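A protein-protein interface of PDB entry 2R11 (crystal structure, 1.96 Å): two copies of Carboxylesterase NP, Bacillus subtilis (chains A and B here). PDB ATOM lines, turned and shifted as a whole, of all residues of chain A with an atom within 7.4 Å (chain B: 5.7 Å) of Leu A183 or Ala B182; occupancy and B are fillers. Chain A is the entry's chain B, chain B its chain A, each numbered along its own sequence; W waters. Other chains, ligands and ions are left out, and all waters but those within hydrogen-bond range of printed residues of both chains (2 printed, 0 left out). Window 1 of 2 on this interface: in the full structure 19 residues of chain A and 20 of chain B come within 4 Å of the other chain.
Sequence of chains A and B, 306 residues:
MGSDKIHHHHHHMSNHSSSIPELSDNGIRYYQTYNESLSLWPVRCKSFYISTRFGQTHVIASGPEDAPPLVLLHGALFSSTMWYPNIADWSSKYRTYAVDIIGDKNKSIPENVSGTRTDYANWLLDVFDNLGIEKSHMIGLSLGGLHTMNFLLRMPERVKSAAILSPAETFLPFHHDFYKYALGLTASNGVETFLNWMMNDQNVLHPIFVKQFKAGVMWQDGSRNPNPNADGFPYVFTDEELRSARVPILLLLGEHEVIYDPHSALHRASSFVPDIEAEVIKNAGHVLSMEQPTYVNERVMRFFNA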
ATOM      1  N   ASP A 177       1.750 -27.062  19.129  1.00  0.00           N
ATOM      2  CA  ASP A 177       1.834 -26.235  20.328  1.00  0.00           C
ATOM      3  C   ASP A 177       0.711 -25.205  20.377  1.00  0.00           C
ATOM      4  O   ASP A 177       0.256 -24.858  21.455  1.00  0.00           O
ATOM      5  CB  ASP A 177       3.187 -25.525  20.433  1.00  0.00           C
ATOM      6  CG  ASP A 177       4.325 -26.475  20.777  1.00  0.00           C
ATOM      7  OD1 ASP A 177       4.058 -27.636  21.158  1.00  0.00           O
ATOM      8  OD2 ASP A 177       5.489 -26.060  20.634  1.00  0.00           O
ATOM      9  N   PHE A 178       0.266 -24.714  19.224  1.00  0.00           N
ATOM     10  CA  PHE A 178      -0.841 -23.765  19.225  1.00  0.00           C
ATOM     11  C   PHE A 178      -2.046 -24.343  19.935  1.00  0.00           C
ATOM     12  O   PHE A 178      -2.682 -23.693  20.790  1.00  0.00           O
ATOM     13  CB  PHE A 178      -1.263 -23.363  17.826  1.00  0.00           C
ATOM     14  CG  PHE A 178      -2.550 -22.594  17.811  1.00  0.00           C
ATOM     15  CD1 PHE A 178      -2.591 -21.283  18.263  1.00  0.00           C
ATOM     16  CD2 PHE A 178      -3.733 -23.192  17.394  1.00  0.00           C
ATOM     17  CE1 PHE A 178      -3.778 -20.569  18.257  1.00  0.00           C
ATOM     18  CE2 PHE A 178      -4.929 -22.476  17.393  1.00  0.00           C
ATOM     19  CZ  PHE A 178      -4.949 -21.166  17.829  1.00  0.00           C
ATOM     20  N   TYR A 179      -2.335 -25.585  19.573  1.00  0.00           N
ATOM     21  CA  TYR A 179      -3.435 -26.332  20.130  1.00  0.00           C
ATOM     22  C   TYR A 179      -3.209 -26.643  21.588  1.00  0.00           C
ATOM     23  O   TYR A 179      -4.114 -26.532  22.383  1.00  0.00           O
ATOM     24  CB  TYR A 179      -3.690 -27.603  19.313  1.00  0.00           C
ATOM     25  CG  TYR A 179      -4.351 -27.342  17.973  1.00  0.00           C
ATOM     26  CD1 TYR A 179      -5.560 -26.663  17.906  1.00  0.00           C
ATOM     27  CD2 TYR A 179      -3.801 -27.808  16.784  1.00  0.00           C
ATOM     28  CE1 TYR A 179      -6.201 -26.426  16.682  1.00  0.00           C
ATOM     29  CE2 TYR A 179      -4.435 -27.573  15.552  1.00  0.00           C
ATOM     30  CZ  TYR A 179      -5.645 -26.888  15.522  1.00  0.00           C
ATOM     31  OH  TYR A 179      -6.295 -26.643  14.340  1.00  0.00           O
ATOM     32  N   LYS A 180      -1.995 -27.015  21.960  1.00  0.00           N
ATOM     33  CA  LYS A 180      -1.721 -27.300  23.359  1.00  0.00           C
ATOM     34  C   LYS A 180      -1.880 -26.054  24.246  1.00  0.00           C
ATOM     35  O   LYS A 180      -2.427 -26.131  25.353  1.00  0.00           O
ATOM     36  CB  LYS A 180      -0.353 -27.948  23.509  1.00  0.00           C
ATOM     37  CG  LYS A 180      -0.325 -29.337  22.902  1.00  0.00           C
ATOM     38  CD  LYS A 180       1.074 -29.871  22.781  1.00  0.00           C
ATOM     39  CE  LYS A 180       1.037 -31.315  22.355  1.00  0.00           C
ATOM     40  NZ  LYS A 180       2.385 -31.838  22.069  1.00  0.00           N
ATOM     41  N   TYR A 181      -1.451 -24.901  23.758  1.00  0.00           N
ATOM     42  CA  TYR A 181      -1.611 -23.683  24.550  1.00  0.00           C
ATOM     43  C   TYR A 181      -3.065 -23.204  24.561  1.00  0.00           C
ATOM     44  O   TYR A 181      -3.568 -22.788  25.589  1.00  0.00           O
ATOM     45  CB  TYR A 181      -0.653 -22.590  24.079  1.00  0.00           C
ATOM     46  CG  TYR A 181       0.738 -22.748  24.659  1.00  0.00           C
ATOM     47  CD1 TYR A 181       1.032 -22.269  25.929  1.00  0.00           C
ATOM     48  CD2 TYR A 181       1.749 -23.378  23.940  1.00  0.00           C
ATOM     49  CE1 TYR A 181       2.308 -22.395  26.467  1.00  0.00           C
ATOM     50  CE2 TYR A 181       3.024 -23.532  24.473  1.00  0.00           C
ATOM     51  CZ  TYR A 181       3.293 -23.036  25.735  1.00  0.00           C
ATOM     52  OH  TYR A 181       4.550 -23.165  26.262  1.00  0.00           O
ATOM     53  N   ALA A 182      -3.719 -23.302  23.413  1.00  0.00           N
ATOM     54  CA  ALA A 182      -5.129 -22.950  23.266  1.00  0.00           C
ATOM     55  C   ALA A 182      -6.014 -23.781  24.225  1.00  0.00           C
ATOM     56  O   ALA A 182      -6.858 -23.245  24.937  1.00  0.00           O
ATOM     57  CB  ALA A 182      -5.536 -23.185  21.878  1.00  0.00           C
ATOM     58  N   LEU A 183      -5.800 -25.091  24.259  1.00  0.00           N
ATOM     59  CA  LEU A 183      -6.588 -25.936  25.158  1.00  0.00           C
ATOM     60  C   LEU A 183      -6.439 -25.516  26.614  1.00  0.00           C
ATOM     61  O   LEU A 183      -7.335 -25.747  27.412  1.00  0.00           O
ATOM     62  CB  LEU A 183      -6.224 -27.401  24.982  1.00  0.00           C
ATOM     63  CG  LEU A 183      -7.010 -28.132  23.906  1.00  0.00           C
ATOM     64  CD1 LEU A 183      -6.389 -29.505  23.619  1.00  0.00           C
ATOM     65  CD2 LEU A 183      -8.467 -28.288  24.347  1.00  0.00           C
ATOM     66  N   GLY A 184      -5.320 -24.894  26.974  1.00  0.00           N
ATOM     67  CA  GLY A 184      -5.135 -24.431  28.352  1.00  0.00           C
ATOM     68  C   GLY A 184      -5.786 -23.097  28.701  1.00  0.00           C
ATOM     69  O   GLY A 184      -5.774 -22.697  29.860  1.00  0.00           O
ATOM     70  N   LEU A 185      -6.339 -22.389  27.709  1.00  0.00           N
ATOM     71  CA  LEU A 185      -6.924 -21.053  27.951  1.00  0.00           C
ATOM     72  C   LEU A 185      -7.925 -21.040  29.108  1.00  0.00           C
ATOM     73  O   LEU A 185      -7.926 -20.112  29.913  1.00  0.00           O
ATOM     74  CB  LEU A 185      -7.572 -20.472  26.670  1.00  0.00           C
ATOM     75  CG  LEU A 185      -6.649 -19.839  25.623  1.00  0.00           C
ATOM     76  CD1 LEU A 185      -7.388 -19.510  24.335  1.00  0.00           C
ATOM     77  CD2 LEU A 185      -5.956 -18.608  26.166  1.00  0.00           C
ATOM     78  N   THR A 186      -8.739 -22.090  29.193  1.00  0.00           N
ATOM     79  CA  THR A 186      -9.786 -22.235  30.223  1.00  0.00           C
ATOM     80  C   THR A 186      -9.270 -23.055  31.407  1.00  0.00           C
ATOM     81  O   THR A 186      -9.704 -24.183  31.667  1.00  0.00           O
ATOM     82  CB  THR A 186     -11.023 -22.911  29.639  1.00  0.00           C
ATOM     83  OG1 THR A 186     -10.613 -24.053  28.874  1.00  0.00           O
ATOM     84  CG2 THR A 186     -11.777 -21.947  28.724  1.00  0.00           C
ATOM     85  N   ALA A 187      -8.313 -22.461  32.101  1.00  0.00           N
ATOM     86  CA  ALA A 187      -7.690 -23.043  33.271  1.00  0.00           C
ATOM     87  C   ALA A 187      -7.159 -21.873  34.046  1.00  0.00           C
ATOM     88  O   ALA A 187      -6.953 -20.777  33.497  1.00  0.00           O
ATOM     89  CB  ALA A 187      -6.556 -23.988  32.890  1.00  0.00           C
ATOM     90  N   GLY A 190      -4.473 -19.737  32.559  1.00  0.00           N
ATOM     91  CA  GLY A 190      -4.411 -20.172  31.179  1.00  0.00           C
ATOM     92  C   GLY A 190      -4.160 -19.071  30.166  1.00  0.00           C
ATOM     93  O   GLY A 190      -3.515 -19.309  29.145  1.00  0.00           O
ATOM     94  N   PHE A 194      -0.943 -18.493  27.840  1.00  0.00           N
ATOM     95  CA  PHE A 194      -1.120 -18.428  26.401  1.00  0.00           C
ATOM     96  C   PHE A 194      -0.447 -17.189  25.868  1.00  0.00           C
ATOM     97  O   PHE A 194       0.334 -17.259  24.919  1.00  0.00           O
ATOM     98  CB  PHE A 194      -2.606 -18.388  26.028  1.00  0.00           C
ATOM     99  CG  PHE A 194      -2.869 -18.356  24.538  1.00  0.00           C
ATOM    100  CD1 PHE A 194      -2.867 -19.528  23.796  1.00  0.00           C
ATOM    101  CD2 PHE A 194      -3.175 -17.165  23.888  1.00  0.00           C
ATOM    102  CE1 PHE A 194      -3.114 -19.509  22.403  1.00  0.00           C
ATOM    103  CE2 PHE A 194      -3.431 -17.141  22.506  1.00  0.00           C
ATOM    104  CZ  PHE A 194      -3.403 -18.314  21.766  1.00  0.00           C
ATOM    105  N   PRO A 228     -16.678 -28.865  13.760  1.00  0.00           N
ATOM    106  CA  PRO A 228     -15.494 -28.984  12.924  1.00  0.00           C
ATOM    107  C   PRO A 228     -15.848 -29.568  11.544  1.00  0.00           C
ATOM    108  O   PRO A 228     -16.788 -30.361  11.429  1.00  0.00           O
ATOM    109  CB  PRO A 228     -14.595 -29.907  13.741  1.00  0.00           C
ATOM    110  CG  PRO A 228     -14.977 -29.594  15.176  1.00  0.00           C
ATOM    111  CD  PRO A 228     -16.443 -29.341  15.134  1.00  0.00           C
ATOM    112  N   ASP B 177      -8.264 -33.019  14.197  1.00  0.00           N
ATOM    113  CA  ASP B 177      -9.678 -33.084  14.560  1.00  0.00           C
ATOM    114  C   ASP B 177      -9.873 -33.205  16.054  1.00  0.00           C
ATOM    115  O   ASP B 177     -10.768 -32.582  16.606  1.00  0.00           O
ATOM    116  CB  ASP B 177     -10.381 -34.255  13.882  1.00  0.00           C
ATOM    117  CG  ASP B 177     -10.816 -33.931  12.470  1.00  0.00           C
ATOM    118  OD1 ASP B 177     -10.617 -32.774  12.026  1.00  0.00           O
ATOM    119  OD2 ASP B 177     -11.363 -34.849  11.821  1.00  0.00           O
ATOM    120  N   PHE B 178      -9.010 -33.971  16.712  1.00  0.00           N
ATOM    121  CA  PHE B 178      -9.119 -34.126  18.157  1.00  0.00           C
ATOM    122  C   PHE B 178      -9.069 -32.751  18.824  1.00  0.00           C
ATOM    123  O   PHE B 178      -9.918 -32.432  19.652  1.00  0.00           O
ATOM    124  CB  PHE B 178      -8.020 -35.042  18.716  1.00  0.00           C
ATOM    125  CG  PHE B 178      -7.857 -34.924  20.207  1.00  0.00           C
ATOM    126  CD1 PHE B 178      -8.860 -35.347  21.054  1.00  0.00           C
ATOM    127  CD2 PHE B 178      -6.738 -34.336  20.753  1.00  0.00           C
ATOM    128  CE1 PHE B 178      -8.727 -35.210  22.420  1.00  0.00           C
ATOM    129  CE2 PHE B 178      -6.601 -34.213  22.110  1.00  0.00           C
ATOM    130  CZ  PHE B 178      -7.590 -34.649  22.942  1.00  0.00           C
ATOM    131  N   TYR B 179      -8.074 -31.948  18.438  1.00  0.00           N
ATOM    132  CA  TYR B 179      -7.885 -30.603  18.993  1.00  0.00           C
ATOM    133  C   TYR B 179      -9.056 -29.654  18.689  1.00  0.00           C
ATOM    134  O   TYR B 179      -9.445 -28.828  19.522  1.00  0.00           O
ATOM    135  CB  TYR B 179      -6.551 -30.005  18.490  1.00  0.00           C
ATOM    136  CG  TYR B 179      -5.309 -30.615  19.143  1.00  0.00           C
ATOM    137  CD1 TYR B 179      -5.150 -30.546  20.519  1.00  0.00           C
ATOM    138  CD2 TYR B 179      -4.287 -31.215  18.388  1.00  0.00           C
ATOM    139  CE1 TYR B 179      -4.046 -31.062  21.139  1.00  0.00           C
ATOM    140  CE2 TYR B 179      -3.146 -31.757  19.017  1.00  0.00           C
ATOM    141  CZ  TYR B 179      -3.048 -31.679  20.404  1.00  0.00           C
ATOM    142  OH  TYR B 179      -1.962 -32.176  21.111  1.00  0.00           O
ATOM    143  N   LYS B 180      -9.607 -29.766  17.488  1.00  0.00           N
ATOM    144  CA  LYS B 180     -10.745 -28.948  17.082  1.00  0.00           C
ATOM    145  C   LYS B 180     -11.970 -29.265  17.942  1.00  0.00           C
ATOM    146  O   LYS B 180     -12.630 -28.351  18.458  1.00  0.00           O
ATOM    147  CB  LYS B 180     -11.017 -29.115  15.581  1.00  0.00           C
ATOM    148  CG  LYS B 180      -9.923 -28.461  14.709  1.00  0.00           C
ATOM    149  CD  LYS B 180      -9.992 -28.849  13.211  1.00  0.00           C
ATOM    150  CE  LYS B 180      -8.817 -28.210  12.445  1.00  0.00           C
ATOM    151  NZ  LYS B 180      -8.765 -28.531  10.984  1.00  0.00           N
ATOM    152  N   TYR B 181     -12.257 -30.547  18.145  1.00  0.00           N
ATOM    153  CA  TYR B 181     -13.364 -30.930  19.024  1.00  0.00           C
ATOM    154  C   TYR B 181     -13.096 -30.635  20.512  1.00  0.00           C
ATOM    155  O   TYR B 181     -13.980 -30.187  21.220  1.00  0.00           O
ATOM    156  CB  TYR B 181     -13.714 -32.412  18.841  1.00  0.00           C
ATOM    157  CG  TYR B 181     -14.526 -32.653  17.626  1.00  0.00           C
ATOM    158  CD1 TYR B 181     -15.915 -32.527  17.667  1.00  0.00           C
ATOM    159  CD2 TYR B 181     -13.928 -32.984  16.415  1.00  0.00           C
ATOM    160  CE1 TYR B 181     -16.672 -32.730  16.534  1.00  0.00           C
ATOM    161  CE2 TYR B 181     -14.679 -33.187  15.274  1.00  0.00           C
ATOM    162  CZ  TYR B 181     -16.046 -33.066  15.340  1.00  0.00           C
ATOM    163  OH  TYR B 181     -16.774 -33.293  14.208  1.00  0.00           O
ATOM    164  N   ALA B 182     -11.877 -30.884  20.975  1.00  0.00           N
ATOM    165  CA  ALA B 182     -11.520 -30.633  22.367  1.00  0.00           C
ATOM    166  C   ALA B 182     -11.631 -29.151  22.701  1.00  0.00           C
ATOM    167  O   ALA B 182     -12.015 -28.812  23.796  1.00  0.00           O
ATOM    168  CB  ALA B 182     -10.118 -31.137  22.676  1.00  0.00           C
ATOM    169  N   LEU B 183     -11.289 -28.281  21.756  1.00  0.00           N
ATOM    170  CA  LEU B 183     -11.340 -26.842  21.987  1.00  0.00           C
ATOM    171  C   LEU B 183     -12.762 -26.323  22.134  1.00  0.00           C
ATOM    172  O   LEU B 183     -12.986 -25.310  22.791  1.00  0.00           O
ATOM    173  CB  LEU B 183     -10.599 -26.077  20.875  1.00  0.00           C
ATOM    174  CG  LEU B 183      -9.092 -25.884  21.087  1.00  0.00           C
ATOM    175  CD1 LEU B 183      -8.424 -25.392  19.816  1.00  0.00           C
ATOM    176  CD2 LEU B 183      -8.824 -24.907  22.240  1.00  0.00           C
ATOM    177  N   GLY B 184     -13.712 -27.014  21.513  1.00  0.00           N
ATOM    178  CA  GLY B 184     -15.109 -26.673  21.614  1.00  0.00           C
ATOM    179  C   GLY B 184     -15.805 -27.303  22.818  1.00  0.00           C
ATOM    180  O   GLY B 184     -16.990 -27.083  22.996  1.00  0.00           O
ATOM    181  N   LEU B 185     -15.092 -28.081  23.642  1.00  0.00           N
ATOM    182  CA  LEU B 185     -15.698 -28.678  24.844  1.00  0.00           C
ATOM    183  C   LEU B 185     -16.386 -27.676  25.766  1.00  0.00           C
ATOM    184  O   LEU B 185     -17.468 -27.960  26.287  1.00  0.00           O
ATOM    185  CB  LEU B 185     -14.656 -29.414  25.698  1.00  0.00           C
ATOM    186  CG  LEU B 185     -14.434 -30.902  25.404  1.00  0.00           C
ATOM    187  CD1 LEU B 185     -13.316 -31.449  26.293  1.00  0.00           C
ATOM    188  CD2 LEU B 185     -15.710 -31.689  25.630  1.00  0.00           C
ATOM    189  N   THR B 186     -15.711 -26.549  25.994  1.00  0.00           N
ATOM    190  CA  THR B 186     -16.155 -25.463  26.876  1.00  0.00           C
ATOM    191  C   THR B 186     -16.968 -24.423  26.114  1.00  0.00           C
ATOM    192  O   THR B 186     -16.606 -23.232  26.085  1.00  0.00           O
ATOM    193  CB  THR B 186     -14.949 -24.728  27.458  1.00  0.00           C
ATOM    194  OG1 THR B 186     -14.140 -24.256  26.369  1.00  0.00           O
ATOM    195  CG2 THR B 186     -14.116 -25.654  28.348  1.00  0.00           C
ATOM    196  N   PHE B 194     -18.628 -33.122  21.351  1.00  0.00           N
ATOM    197  CA  PHE B 194     -17.386 -33.858  21.536  1.00  0.00           C
ATOM    198  C   PHE B 194     -17.654 -35.350  21.642  1.00  0.00           C
ATOM    199  O   PHE B 194     -17.045 -36.145  20.920  1.00  0.00           O
ATOM    200  CB  PHE B 194     -16.673 -33.364  22.818  1.00  0.00           C
ATOM    201  CG  PHE B 194     -15.366 -34.072  23.113  1.00  0.00           C
ATOM    202  CD1 PHE B 194     -14.173 -33.654  22.524  1.00  0.00           C
ATOM    203  CD2 PHE B 194     -15.330 -35.132  23.996  1.00  0.00           C
ATOM    204  CE1 PHE B 194     -12.970 -34.302  22.805  1.00  0.00           C
ATOM    205  CE2 PHE B 194     -14.122 -35.787  24.290  1.00  0.00           C
ATOM    206  CZ  PHE B 194     -12.945 -35.369  23.697  1.00  0.00           C
ATOM    207  N   ASN B 225      -2.319 -26.315  35.114  1.00  0.00           N
ATOM    208  CA  ASN B 225      -1.711 -27.319  34.250  1.00  0.00           C
ATOM    209  C   ASN B 225      -0.225 -27.008  34.161  1.00  0.00           C
ATOM    210  O   ASN B 225       0.162 -25.841  34.217  1.00  0.00           O
ATOM    211  CB  ASN B 225      -2.305 -27.272  32.835  1.00  0.00           C
ATOM    212  CG  ASN B 225      -3.765 -27.694  32.785  1.00  0.00           C
ATOM    213  OD1 ASN B 225      -4.189 -28.593  33.512  1.00  0.00           O
ATOM    214  ND2 ASN B 225      -4.534 -27.061  31.902  1.00  0.00           N
HETATM  215  O   HOH W   1     -15.768 -33.633  11.974  1.00  0.00           O
HETATM  216  O   HOH W   2      -3.514 -23.896  31.218  1.00  0.00           O
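CG of Tyr B179 touches CB of Tyr A179, at 3.4 Å. OH of Tyr A179 touches CE of Lys B180, at 3.5 Å. CD1 of Leu B183 touches CD1 of Tyr A179, 3.7 Å away. CE of Lys A180 touches OH of Tyr B179, at 3.4 Å. CD1 of Leu A183 touches CD1 of Tyr B179, at 3.5 Å. Leu A183 touches Ala B182. N of Leu A183 touches CD2 of Leu B183, at 3.6 Å. OG1 of Thr A186 touches CG2 of Thr B186, at 3.9 Å. Ala A187 touches Asn B225. Pro A228 touches Tyr B181.
Leu A183 touches just these residues of chain B: Tyr B179 (3.5 Å), Ala B182 (3.6 Å) and Leu B183 (3.6 Å). Ala B182 touches just one residue of chain A: Leu A183 (3.6 Å). Printed residues of chain B within 4 Å of Ala A187: Asn B225 (3.8 Å). Printed residues of chain B within 4 Å of Thr A186: Thr B186. Of the printed residues of chain B, Lys A180 touches Tyr B179. Of the printed residues of chain B, Ala A182 touches Leu B183. Printed residues of chain B within 4 Å of Tyr A179: Tyr B179, Lys B180 and Leu B183. The nearest residue of chain A that does not touch Ala B182 is Pro A228 (6.7 Å).
Printed residues of chain A that touch a printed residue of chain B: Tyr A179, Lys A180, Ala A182, Leu A183, Thr A186, Ala A187 and Pro A228. Hydrophobic or aromatic side chains of chain A within 4 Å of the printed part of chain B: Tyr A179, Ala A182, Leu A183, Ala A187 and Pro A228. Of the 12 printed residues of chain B, 7 touch a printed residue of chain A. Among the printed residues, 11 pairs touch across the chains.
Tyr B179 touches its own counterpart, Tyr A179. Tyr A179 touches Lys B180, and with the chains exchanged Lys A180 touches Tyr B179. Ala A182 touches Leu B183, and with the chains exchanged Leu A183 touches Ala B182. Leu A183 touches its own counterpart, Leu B183.
Water W1 lies within hydrogen-bond range of the side-chain hydroxyl (OH) of Tyr B181 (2.5 Å) and the backbone carbonyl oxygen (O) of Pro A228 (3.5 Å). Water W2 lies within hydrogen-bond range of O of Gly A184 (2.9 Å) and ND2 of Asn B225 (3.4 Å).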
